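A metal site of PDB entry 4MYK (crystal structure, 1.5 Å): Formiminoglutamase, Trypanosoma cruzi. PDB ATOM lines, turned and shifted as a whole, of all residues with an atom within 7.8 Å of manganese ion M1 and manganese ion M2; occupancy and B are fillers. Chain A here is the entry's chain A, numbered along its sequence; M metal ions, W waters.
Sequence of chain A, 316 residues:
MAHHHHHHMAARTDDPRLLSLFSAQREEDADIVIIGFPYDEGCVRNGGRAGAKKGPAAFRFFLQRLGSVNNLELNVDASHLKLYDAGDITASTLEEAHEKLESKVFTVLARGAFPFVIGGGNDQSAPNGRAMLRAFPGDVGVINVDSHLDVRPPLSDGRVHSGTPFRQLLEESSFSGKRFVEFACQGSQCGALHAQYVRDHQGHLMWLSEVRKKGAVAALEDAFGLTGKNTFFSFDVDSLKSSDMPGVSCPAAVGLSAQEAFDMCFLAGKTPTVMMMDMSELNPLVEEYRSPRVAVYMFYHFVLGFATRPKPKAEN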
ATOM      1  N   GLY A  42     -10.447  28.404  33.434  1.00  0.00           N
ATOM      2  CA  GLY A  42      -9.159  28.240  32.796  1.00  0.00           C
ATOM      3  C   GLY A  42      -9.045  29.283  31.703  1.00  0.00           C
ATOM      4  O   GLY A  42      -9.119  30.475  31.964  1.00  0.00           O
ATOM      5  N   CYS A  43      -8.897  28.827  30.458  1.00  0.00           N
ATOM      6  CA  CYS A  43      -8.670  29.733  29.332  1.00  0.00           C
ATOM      7  C   CYS A  43      -9.901  30.561  28.941  1.00  0.00           C
ATOM      8  O   CYS A  43      -9.788  31.563  28.221  1.00  0.00           O
ATOM      9  CB  CYS A  43      -8.131  28.961  28.128  1.00  0.00           C
ATOM     10  SG  CYS A  43      -7.238  29.999  26.972  1.00  0.00           S
ATOM     11  N   ASN A  46      -8.979  33.923  29.741  1.00  0.00           N
ATOM     12  CA  ASN A  46      -8.106  34.614  28.807  1.00  0.00           C
ATOM     13  C   ASN A  46      -8.662  34.604  27.378  1.00  0.00           C
ATOM     14  O   ASN A  46      -7.975  34.224  26.434  1.00  0.00           O
ATOM     15  CB  ASN A  46      -6.709  33.998  28.827  1.00  0.00           C
ATOM     16  CG  ASN A  46      -6.195  33.771  30.226  1.00  0.00           C
ATOM     17  OD1 ASN A  46      -6.090  34.715  31.020  1.00  0.00           O
ATOM     18  ND2 ASN A  46      -5.876  32.522  30.565  1.00  0.00           N
ATOM     19  N   GLY A 121     -11.624  23.053  32.730  1.00  0.00           N
ATOM     20  CA  GLY A 121     -10.566  23.998  32.381  1.00  0.00           C
ATOM     21  C   GLY A 121      -9.225  23.801  33.081  1.00  0.00           C
ATOM     22  O   GLY A 121      -9.112  23.044  34.029  1.00  0.00           O
ATOM     23  N   ASN A 122      -8.205  24.518  32.591  1.00  0.00           N
ATOM     24  CA  ASN A 122      -6.816  24.434  33.074  1.00  0.00           C
ATOM     25  C   ASN A 122      -6.672  24.388  34.596  1.00  0.00           C
ATOM     26  O   ASN A 122      -5.709  23.793  35.120  1.00  0.00           O
ATOM     27  CB  ASN A 122      -6.006  25.655  32.599  1.00  0.00           C
ATOM     28  CG  ASN A 122      -5.831  25.702  31.085  1.00  0.00           C
ATOM     29  OD1 ASN A 122      -5.574  24.690  30.423  1.00  0.00           O
ATOM     30  ND2 ASN A 122      -5.929  26.902  30.525  1.00  0.00           N
ATOM     31  N   ASP A 123      -7.603  25.025  35.285  1.00  0.00           N
ATOM     32  CA  ASP A 123      -7.468  25.288  36.724  1.00  0.00           C
ATOM     33  C   ASP A 123      -7.411  24.020  37.591  1.00  0.00           C
ATOM     34  O   ASP A 123      -6.888  24.040  38.696  1.00  0.00           O
ATOM     35  CB  ASP A 123      -8.541  26.259  37.195  1.00  0.00           C
ATOM     36  CG  ASP A 123      -8.328  27.674  36.662  1.00  0.00           C
ATOM     37  OD1 ASP A 123      -9.108  28.578  37.046  1.00  0.00           O
ATOM     38  OD2 ASP A 123      -7.390  27.889  35.869  1.00  0.00           O
ATOM     39  N   SER A 125      -5.499  21.729  37.233  1.00  0.00           N
ATOM     40  CA  SER A 125      -4.112  21.295  37.316  1.00  0.00           C
ATOM     41  C   SER A 125      -3.468  21.673  38.635  1.00  0.00           C
ATOM     42  O   SER A 125      -2.539  21.007  39.084  1.00  0.00           O
ATOM     43  CB  SER A 125      -3.308  21.882  36.159  1.00  0.00           C
ATOM     44  OG  SER A 125      -3.967  21.652  34.928  1.00  0.00           O
ATOM     45  N   ASN A 144       3.775  20.906  31.511  1.00  0.00           N
ATOM     46  CA  ASN A 144       2.582  21.546  30.980  1.00  0.00           C
ATOM     47  C   ASN A 144       2.662  21.606  29.448  1.00  0.00           C
ATOM     48  O   ASN A 144       3.394  22.432  28.880  1.00  0.00           O
ATOM     49  CB  ASN A 144       2.398  22.950  31.591  1.00  0.00           C
ATOM     50  CG  ASN A 144       1.132  23.679  31.109  1.00  0.00           C
ATOM     51  OD1 ASN A 144       0.132  23.055  30.762  1.00  0.00           O
ATOM     52  ND2 ASN A 144       1.185  25.002  31.088  1.00  0.00           N
ATOM     53  N   VAL A 145       1.918  20.701  28.803  1.00  0.00           N
ATOM     54  CA  VAL A 145       1.690  20.736  27.360  1.00  0.00           C
ATOM     55  C   VAL A 145       0.569  21.732  27.079  1.00  0.00           C
ATOM     56  O   VAL A 145      -0.602  21.485  27.435  1.00  0.00           O
ATOM     57  CB  VAL A 145       1.286  19.355  26.786  1.00  0.00           C
ATOM     58  CG1 VAL A 145       1.117  19.431  25.253  1.00  0.00           C
ATOM     59  CG2 VAL A 145       2.313  18.292  27.186  1.00  0.00           C
ATOM     60  N   ASP A 146       0.917  22.862  26.466  1.00  0.00           N
ATOM     61  CA  ASP A 146       0.020  23.985  26.418  1.00  0.00           C
ATOM     62  C   ASP A 146       0.577  25.018  25.462  1.00  0.00           C
ATOM     63  O   ASP A 146       1.764  25.328  25.521  1.00  0.00           O
ATOM     64  CB  ASP A 146      -0.083  24.576  27.823  1.00  0.00           C
ATOM     65  CG  ASP A 146      -1.257  25.492  27.983  1.00  0.00           C
ATOM     66  OD1 ASP A 146      -1.879  25.852  26.956  1.00  0.00           O
ATOM     67  OD2 ASP A 146      -1.545  25.853  29.128  1.00  0.00           O
ATOM     68  N   SER A 147      -0.266  25.520  24.563  1.00  0.00           N
ATOM     69  CA  SER A 147       0.136  26.586  23.641  1.00  0.00           C
ATOM     70  C   SER A 147       0.286  27.884  24.409  1.00  0.00           C
ATOM     71  O   SER A 147       0.853  28.855  23.922  1.00  0.00           O
ATOM     72  CB  SER A 147      -0.862  26.739  22.492  1.00  0.00           C
ATOM     73  OG  SER A 147      -2.141  27.118  22.942  1.00  0.00           O
ATOM     74  N   HIS A 148      -0.253  27.885  25.621  1.00  0.00           N
ATOM     75  CA  HIS A 148      -0.240  29.047  26.496  1.00  0.00           C
ATOM     76  C   HIS A 148       0.773  28.851  27.623  1.00  0.00           C
ATOM     77  O   HIS A 148       1.036  27.735  28.081  1.00  0.00           O
ATOM     78  CB  HIS A 148      -1.643  29.322  27.079  1.00  0.00           C
ATOM     79  CG  HIS A 148      -2.700  29.537  26.034  1.00  0.00           C
ATOM     80  ND1 HIS A 148      -3.664  28.600  25.755  1.00  0.00           N
ATOM     81  CD2 HIS A 148      -2.927  30.567  25.191  1.00  0.00           C
ATOM     82  CE1 HIS A 148      -4.451  29.042  24.796  1.00  0.00           C
ATOM     83  NE2 HIS A 148      -4.020  30.235  24.436  1.00  0.00           N
ATOM     84  N   LEU A 149       1.349  29.973  28.036  1.00  0.00           N
ATOM     85  CA  LEU A 149       2.220  30.033  29.186  1.00  0.00           C
ATOM     86  C   LEU A 149       1.699  31.206  30.006  1.00  0.00           C
ATOM     87  O   LEU A 149       2.140  32.343  29.860  1.00  0.00           O
ATOM     88  CB  LEU A 149       3.661  30.225  28.716  1.00  0.00           C
ATOM     89  CG  LEU A 149       4.716  30.975  29.530  1.00  0.00           C
ATOM     90  CD1 LEU A 149       4.575  30.759  31.032  1.00  0.00           C
ATOM     91  CD2 LEU A 149       6.108  30.581  29.023  1.00  0.00           C
ATOM     92  N   ASP A 150       0.715  30.909  30.857  1.00  0.00           N
ATOM     93  CA  ASP A 150      -0.011  31.912  31.629  1.00  0.00           C
ATOM     94  C   ASP A 150       0.230  31.714  33.116  1.00  0.00           C
ATOM     95  O   ASP A 150      -0.268  30.762  33.723  1.00  0.00           O
ATOM     96  CB  ASP A 150      -1.503  31.838  31.306  1.00  0.00           C
ATOM     97  CG  ASP A 150      -2.305  32.928  31.982  1.00  0.00           C
ATOM     98  OD1 ASP A 150      -1.764  33.602  32.884  1.00  0.00           O
ATOM     99  OD2 ASP A 150      -3.477  33.112  31.612  1.00  0.00           O
ATOM    100  N   PRO A 165      -2.923  28.009  37.208  1.00  0.00           N
ATOM    101  CA  PRO A 165      -2.567  26.785  37.962  1.00  0.00           C
ATOM    102  C   PRO A 165      -1.064  26.550  38.202  1.00  0.00           C
ATOM    103  O   PRO A 165      -0.696  25.945  39.210  1.00  0.00           O
ATOM    104  CB  PRO A 165      -3.149  25.655  37.103  1.00  0.00           C
ATOM    105  CG  PRO A 165      -3.423  26.274  35.758  1.00  0.00           C
ATOM    106  CD  PRO A 165      -3.722  27.710  36.017  1.00  0.00           C
ATOM    107  N   PHE A 166      -0.212  27.009  37.289  1.00  0.00           N
ATOM    108  CA  PHE A 166       1.202  26.660  37.389  1.00  0.00           C
ATOM    109  C   PHE A 166       2.003  27.711  38.124  1.00  0.00           C
ATOM    110  O   PHE A 166       3.101  27.452  38.618  1.00  0.00           O
ATOM    111  CB  PHE A 166       1.760  26.311  36.012  1.00  0.00           C
ATOM    112  CG  PHE A 166       1.134  25.077  35.433  1.00  0.00           C
ATOM    113  CD1 PHE A 166       1.396  23.838  35.976  1.00  0.00           C
ATOM    114  CD2 PHE A 166       0.222  25.169  34.395  1.00  0.00           C
ATOM    115  CE1 PHE A 166       0.815  22.712  35.480  1.00  0.00           C
ATOM    116  CE2 PHE A 166      -0.378  24.018  33.895  1.00  0.00           C
ATOM    117  CZ  PHE A 166      -0.070  22.798  34.427  1.00  0.00           C
ATOM    118  N   GLU A 182       7.426  23.796  30.262  1.00  0.00           N
ATOM    119  CA  GLU A 182       6.342  24.300  29.431  1.00  0.00           C
ATOM    120  C   GLU A 182       6.600  23.714  28.061  1.00  0.00           C
ATOM    121  O   GLU A 182       7.631  23.992  27.449  1.00  0.00           O
ATOM    122  CB  GLU A 182       6.369  25.824  29.355  1.00  0.00           C
ATOM    123  CG  GLU A 182       6.184  26.529  30.703  1.00  0.00           C
ATOM    124  CD  GLU A 182       4.726  26.687  31.100  1.00  0.00           C
ATOM    125  OE1 GLU A 182       3.862  25.931  30.605  1.00  0.00           O
ATOM    126  OE2 GLU A 182       4.430  27.585  31.916  1.00  0.00           O
ATOM    127  N   GLN A 189       1.792  33.993  21.900  1.00  0.00           N
ATOM    128  CA  GLN A 189       0.792  33.917  22.958  1.00  0.00           C
ATOM    129  C   GLN A 189       1.415  33.863  24.334  1.00  0.00           C
ATOM    130  O   GLN A 189       0.751  33.442  25.288  1.00  0.00           O
ATOM    131  CB  GLN A 189      -0.029  32.629  22.811  1.00  0.00           C
ATOM    132  CG  GLN A 189      -1.018  32.612  21.694  1.00  0.00           C
ATOM    133  CD  GLN A 189      -2.172  31.684  22.005  1.00  0.00           C
ATOM    134  OE1 GLN A 189      -3.335  32.086  21.932  1.00  0.00           O
ATOM    135  NE2 GLN A 189      -1.853  30.447  22.388  1.00  0.00           N
ATOM    136  N   SER A 234       0.526  16.818  32.204  1.00  0.00           N
ATOM    137  CA  SER A 234      -0.624  17.726  32.091  1.00  0.00           C
ATOM    138  C   SER A 234      -0.797  18.172  30.644  1.00  0.00           C
ATOM    139  O   SER A 234       0.052  18.883  30.089  1.00  0.00           O
ATOM    140  CB  SER A 234      -0.420  18.948  32.991  1.00  0.00           C
ATOM    141  OG  SER A 234      -1.588  19.749  33.072  1.00  0.00           O
ATOM    142  N   PHE A 235      -1.892  17.750  30.024  1.00  0.00           N
ATOM    143  CA  PHE A 235      -2.077  17.961  28.596  1.00  0.00           C
ATOM    144  C   PHE A 235      -3.227  18.890  28.261  1.00  0.00           C
ATOM    145  O   PHE A 235      -4.363  18.440  28.123  1.00  0.00           O
ATOM    146  CB  PHE A 235      -2.310  16.636  27.883  1.00  0.00           C
ATOM    147  CG  PHE A 235      -1.820  16.629  26.457  1.00  0.00           C
ATOM    148  CD1 PHE A 235      -2.118  17.673  25.604  1.00  0.00           C
ATOM    149  CD2 PHE A 235      -1.048  15.577  25.968  1.00  0.00           C
ATOM    150  CE1 PHE A 235      -1.680  17.669  24.299  1.00  0.00           C
ATOM    151  CE2 PHE A 235      -0.601  15.570  24.660  1.00  0.00           C
ATOM    152  CZ  PHE A 235      -0.916  16.615  23.831  1.00  0.00           C
ATOM    153  N   ASP A 236      -2.942  20.186  28.106  1.00  0.00           N
ATOM    154  CA  ASP A 236      -3.954  21.132  27.627  1.00  0.00           C
ATOM    155  C   ASP A 236      -4.174  20.850  26.151  1.00  0.00           C
ATOM    156  O   ASP A 236      -3.237  20.947  25.362  1.00  0.00           O
ATOM    157  CB  ASP A 236      -3.501  22.569  27.837  1.00  0.00           C
ATOM    158  CG  ASP A 236      -4.535  23.601  27.390  1.00  0.00           C
ATOM    159  OD1 ASP A 236      -5.403  23.300  26.536  1.00  0.00           O
ATOM    160  OD2 ASP A 236      -4.498  24.726  27.913  1.00  0.00           O
ATOM    161  N   VAL A 237      -5.398  20.498  25.767  1.00  0.00           N
ATOM    162  CA  VAL A 237      -5.639  20.087  24.388  1.00  0.00           C
ATOM    163  C   VAL A 237      -5.693  21.263  23.385  1.00  0.00           C
ATOM    164  O   VAL A 237      -5.716  21.040  22.160  1.00  0.00           O
ATOM    165  CB  VAL A 237      -6.855  19.138  24.257  1.00  0.00           C
ATOM    166  CG1 VAL A 237      -6.597  17.841  24.993  1.00  0.00           C
ATOM    167  CG2 VAL A 237      -8.129  19.794  24.759  1.00  0.00           C
ATOM    168  N   ASP A 238      -5.700  22.504  23.888  1.00  0.00           N
ATOM    169  CA  ASP A 238      -5.621  23.665  23.012  1.00  0.00           C
ATOM    170  C   ASP A 238      -4.184  23.912  22.545  1.00  0.00           C
ATOM    171  O   ASP A 238      -3.867  24.934  21.931  1.00  0.00           O
ATOM    172  CB  ASP A 238      -6.271  24.908  23.635  1.00  0.00           C
ATOM    173  CG  ASP A 238      -5.411  25.564  24.706  1.00  0.00           C
ATOM    174  OD1 ASP A 238      -4.186  25.318  24.756  1.00  0.00           O
ATOM    175  OD2 ASP A 238      -5.971  26.359  25.505  1.00  0.00           O
ATOM    176  N   SER A 239      -3.311  22.948  22.860  1.00  0.00           N
ATOM    177  CA  SER A 239      -1.945  22.920  22.327  1.00  0.00           C
ATOM    178  C   SER A 239      -1.895  22.231  20.956  1.00  0.00           C
ATOM    179  O   SER A 239      -0.856  22.206  20.293  1.00  0.00           O
ATOM    180  CB  SER A 239      -1.041  22.180  23.299  1.00  0.00           C
ATOM    181  OG  SER A 239      -1.439  20.826  23.390  1.00  0.00           O
ATOM    182  N   VAL A 248     -12.191  23.424  21.672  1.00  0.00           N
ATOM    183  CA  VAL A 248     -11.485  23.824  22.886  1.00  0.00           C
ATOM    184  C   VAL A 248     -11.868  25.268  23.135  1.00  0.00           C
ATOM    185  O   VAL A 248     -12.450  25.895  22.258  1.00  0.00           O
ATOM    186  CB  VAL A 248      -9.935  23.678  22.760  1.00  0.00           C
ATOM    187  CG1 VAL A 248      -9.544  22.253  22.401  1.00  0.00           C
ATOM    188  CG2 VAL A 248      -9.372  24.656  21.750  1.00  0.00           C
ATOM    189  N   CYS A 250      -9.895  27.900  23.789  1.00  0.00           N
ATOM    190  CA  CYS A 250      -8.987  28.793  23.084  1.00  0.00           C
ATOM    191  C   CYS A 250      -8.366  28.076  21.894  1.00  0.00           C
ATOM    192  O   CYS A 250      -7.248  27.592  21.973  1.00  0.00           O
ATOM    193  CB  CYS A 250      -7.882  29.277  24.027  1.00  0.00           C
ATOM    194  SG  CYS A 250      -8.470  30.335  25.385  1.00  0.00           S
ATOM    195  N   SER A 280      -6.954  18.998  29.723  1.00  0.00           N
ATOM    196  CA  SER A 280      -7.704  20.227  29.982  1.00  0.00           C
ATOM    197  C   SER A 280      -8.228  20.878  28.723  1.00  0.00           C
ATOM    198  O   SER A 280      -7.662  20.702  27.652  1.00  0.00           O
ATOM    199  CB  SER A 280      -6.810  21.239  30.708  1.00  0.00           C
ATOM    200  OG  SER A 280      -6.679  20.920  32.065  1.00  0.00           O
ATOM    201  N   GLU A 281      -9.311  21.637  28.878  1.00  0.00           N
ATOM    202  CA  GLU A 281      -9.808  22.591  27.882  1.00  0.00           C
ATOM    203  C   GLU A 281     -10.723  22.024  26.775  1.00  0.00           C
ATOM    204  O   GLU A 281     -11.099  22.733  25.854  1.00  0.00           O
ATOM    205  CB  GLU A 281      -8.661  23.435  27.304  1.00  0.00           C
ATOM    206  CG  GLU A 281      -7.958  24.327  28.353  1.00  0.00           C
ATOM    207  CD  GLU A 281      -8.882  25.409  28.886  1.00  0.00           C
ATOM    208  OE1 GLU A 281      -9.802  25.811  28.137  1.00  0.00           O
ATOM    209  OE2 GLU A 281      -8.700  25.863  30.033  1.00  0.00           O
HETATM  210 MN    MN M   1      -3.932  26.536  26.691  1.00  0.00          MN
HETATM  211 MN    MN M   2      -3.556  26.165  29.547  1.00  0.00          MN
HETATM  212  O   HOH W   1      -2.532  25.520  31.859  1.00  0.00           O
HETATM  213  O   HOH W   2      -4.544  27.819  28.630  1.00  0.00           O
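The side-chain carboxylate (OD2) of Asp 146 lies close to the side-chain amide nitrogen (ND2) of Asn 144.
The backbone carbonyl oxygen (O) of Asp 236 is in hydrogen-bond range of the side-chain hydroxyl (OG) of Ser 239 (2.7 Å).
The backbone NH (N) of Asp 236 lies within hydrogen-bond range of the backbone carbonyl oxygen (O) of Val 145.
NE2 of His 148 sits at hydrogen-bond distance from NE2 of Gln 189 (3.0 Å).
The backbone carbonyl oxygen (O) of Asp 238 is in hydrogen-bond range of the side-chain hydroxyl (OG) of Ser 147 (3.0 Å).
The side-chain carboxylate of Glu 281 is in hydrogen-bond range of the backbone NH of Asn 122 (2.9 Å).
The backbone carbonyl oxygen (O) of Asn 122 lies within hydrogen-bond range of the side-chain hydroxyl (OG) of Ser 125 (2.8 Å).
SG of Cys 43 is disulfide-bonded to SG of Cys 250 (2.0 Å).
The nearest printed residue that does not touch manganese ion M1 is Ser 147 (4.2 Å).
Of the 28 residues printed, 3 come within 4 Å of manganese ion M2.
The nearest printed residue that does not touch manganese ion M2 is His 148 (4.4 Å).
Manganese ion M1 is bound by OD1 of Asp 146, OD2 of Asp 236, ND1 of His 148, OD1 of Asp 238, OD2 of Asp 238 and water W2.
Manganese ion M2 is bound by OD2 of Asp 146, water W2, OD2 of Asp 236, water W1, OD1 of Asn 122 and ND2 of Asn 122.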
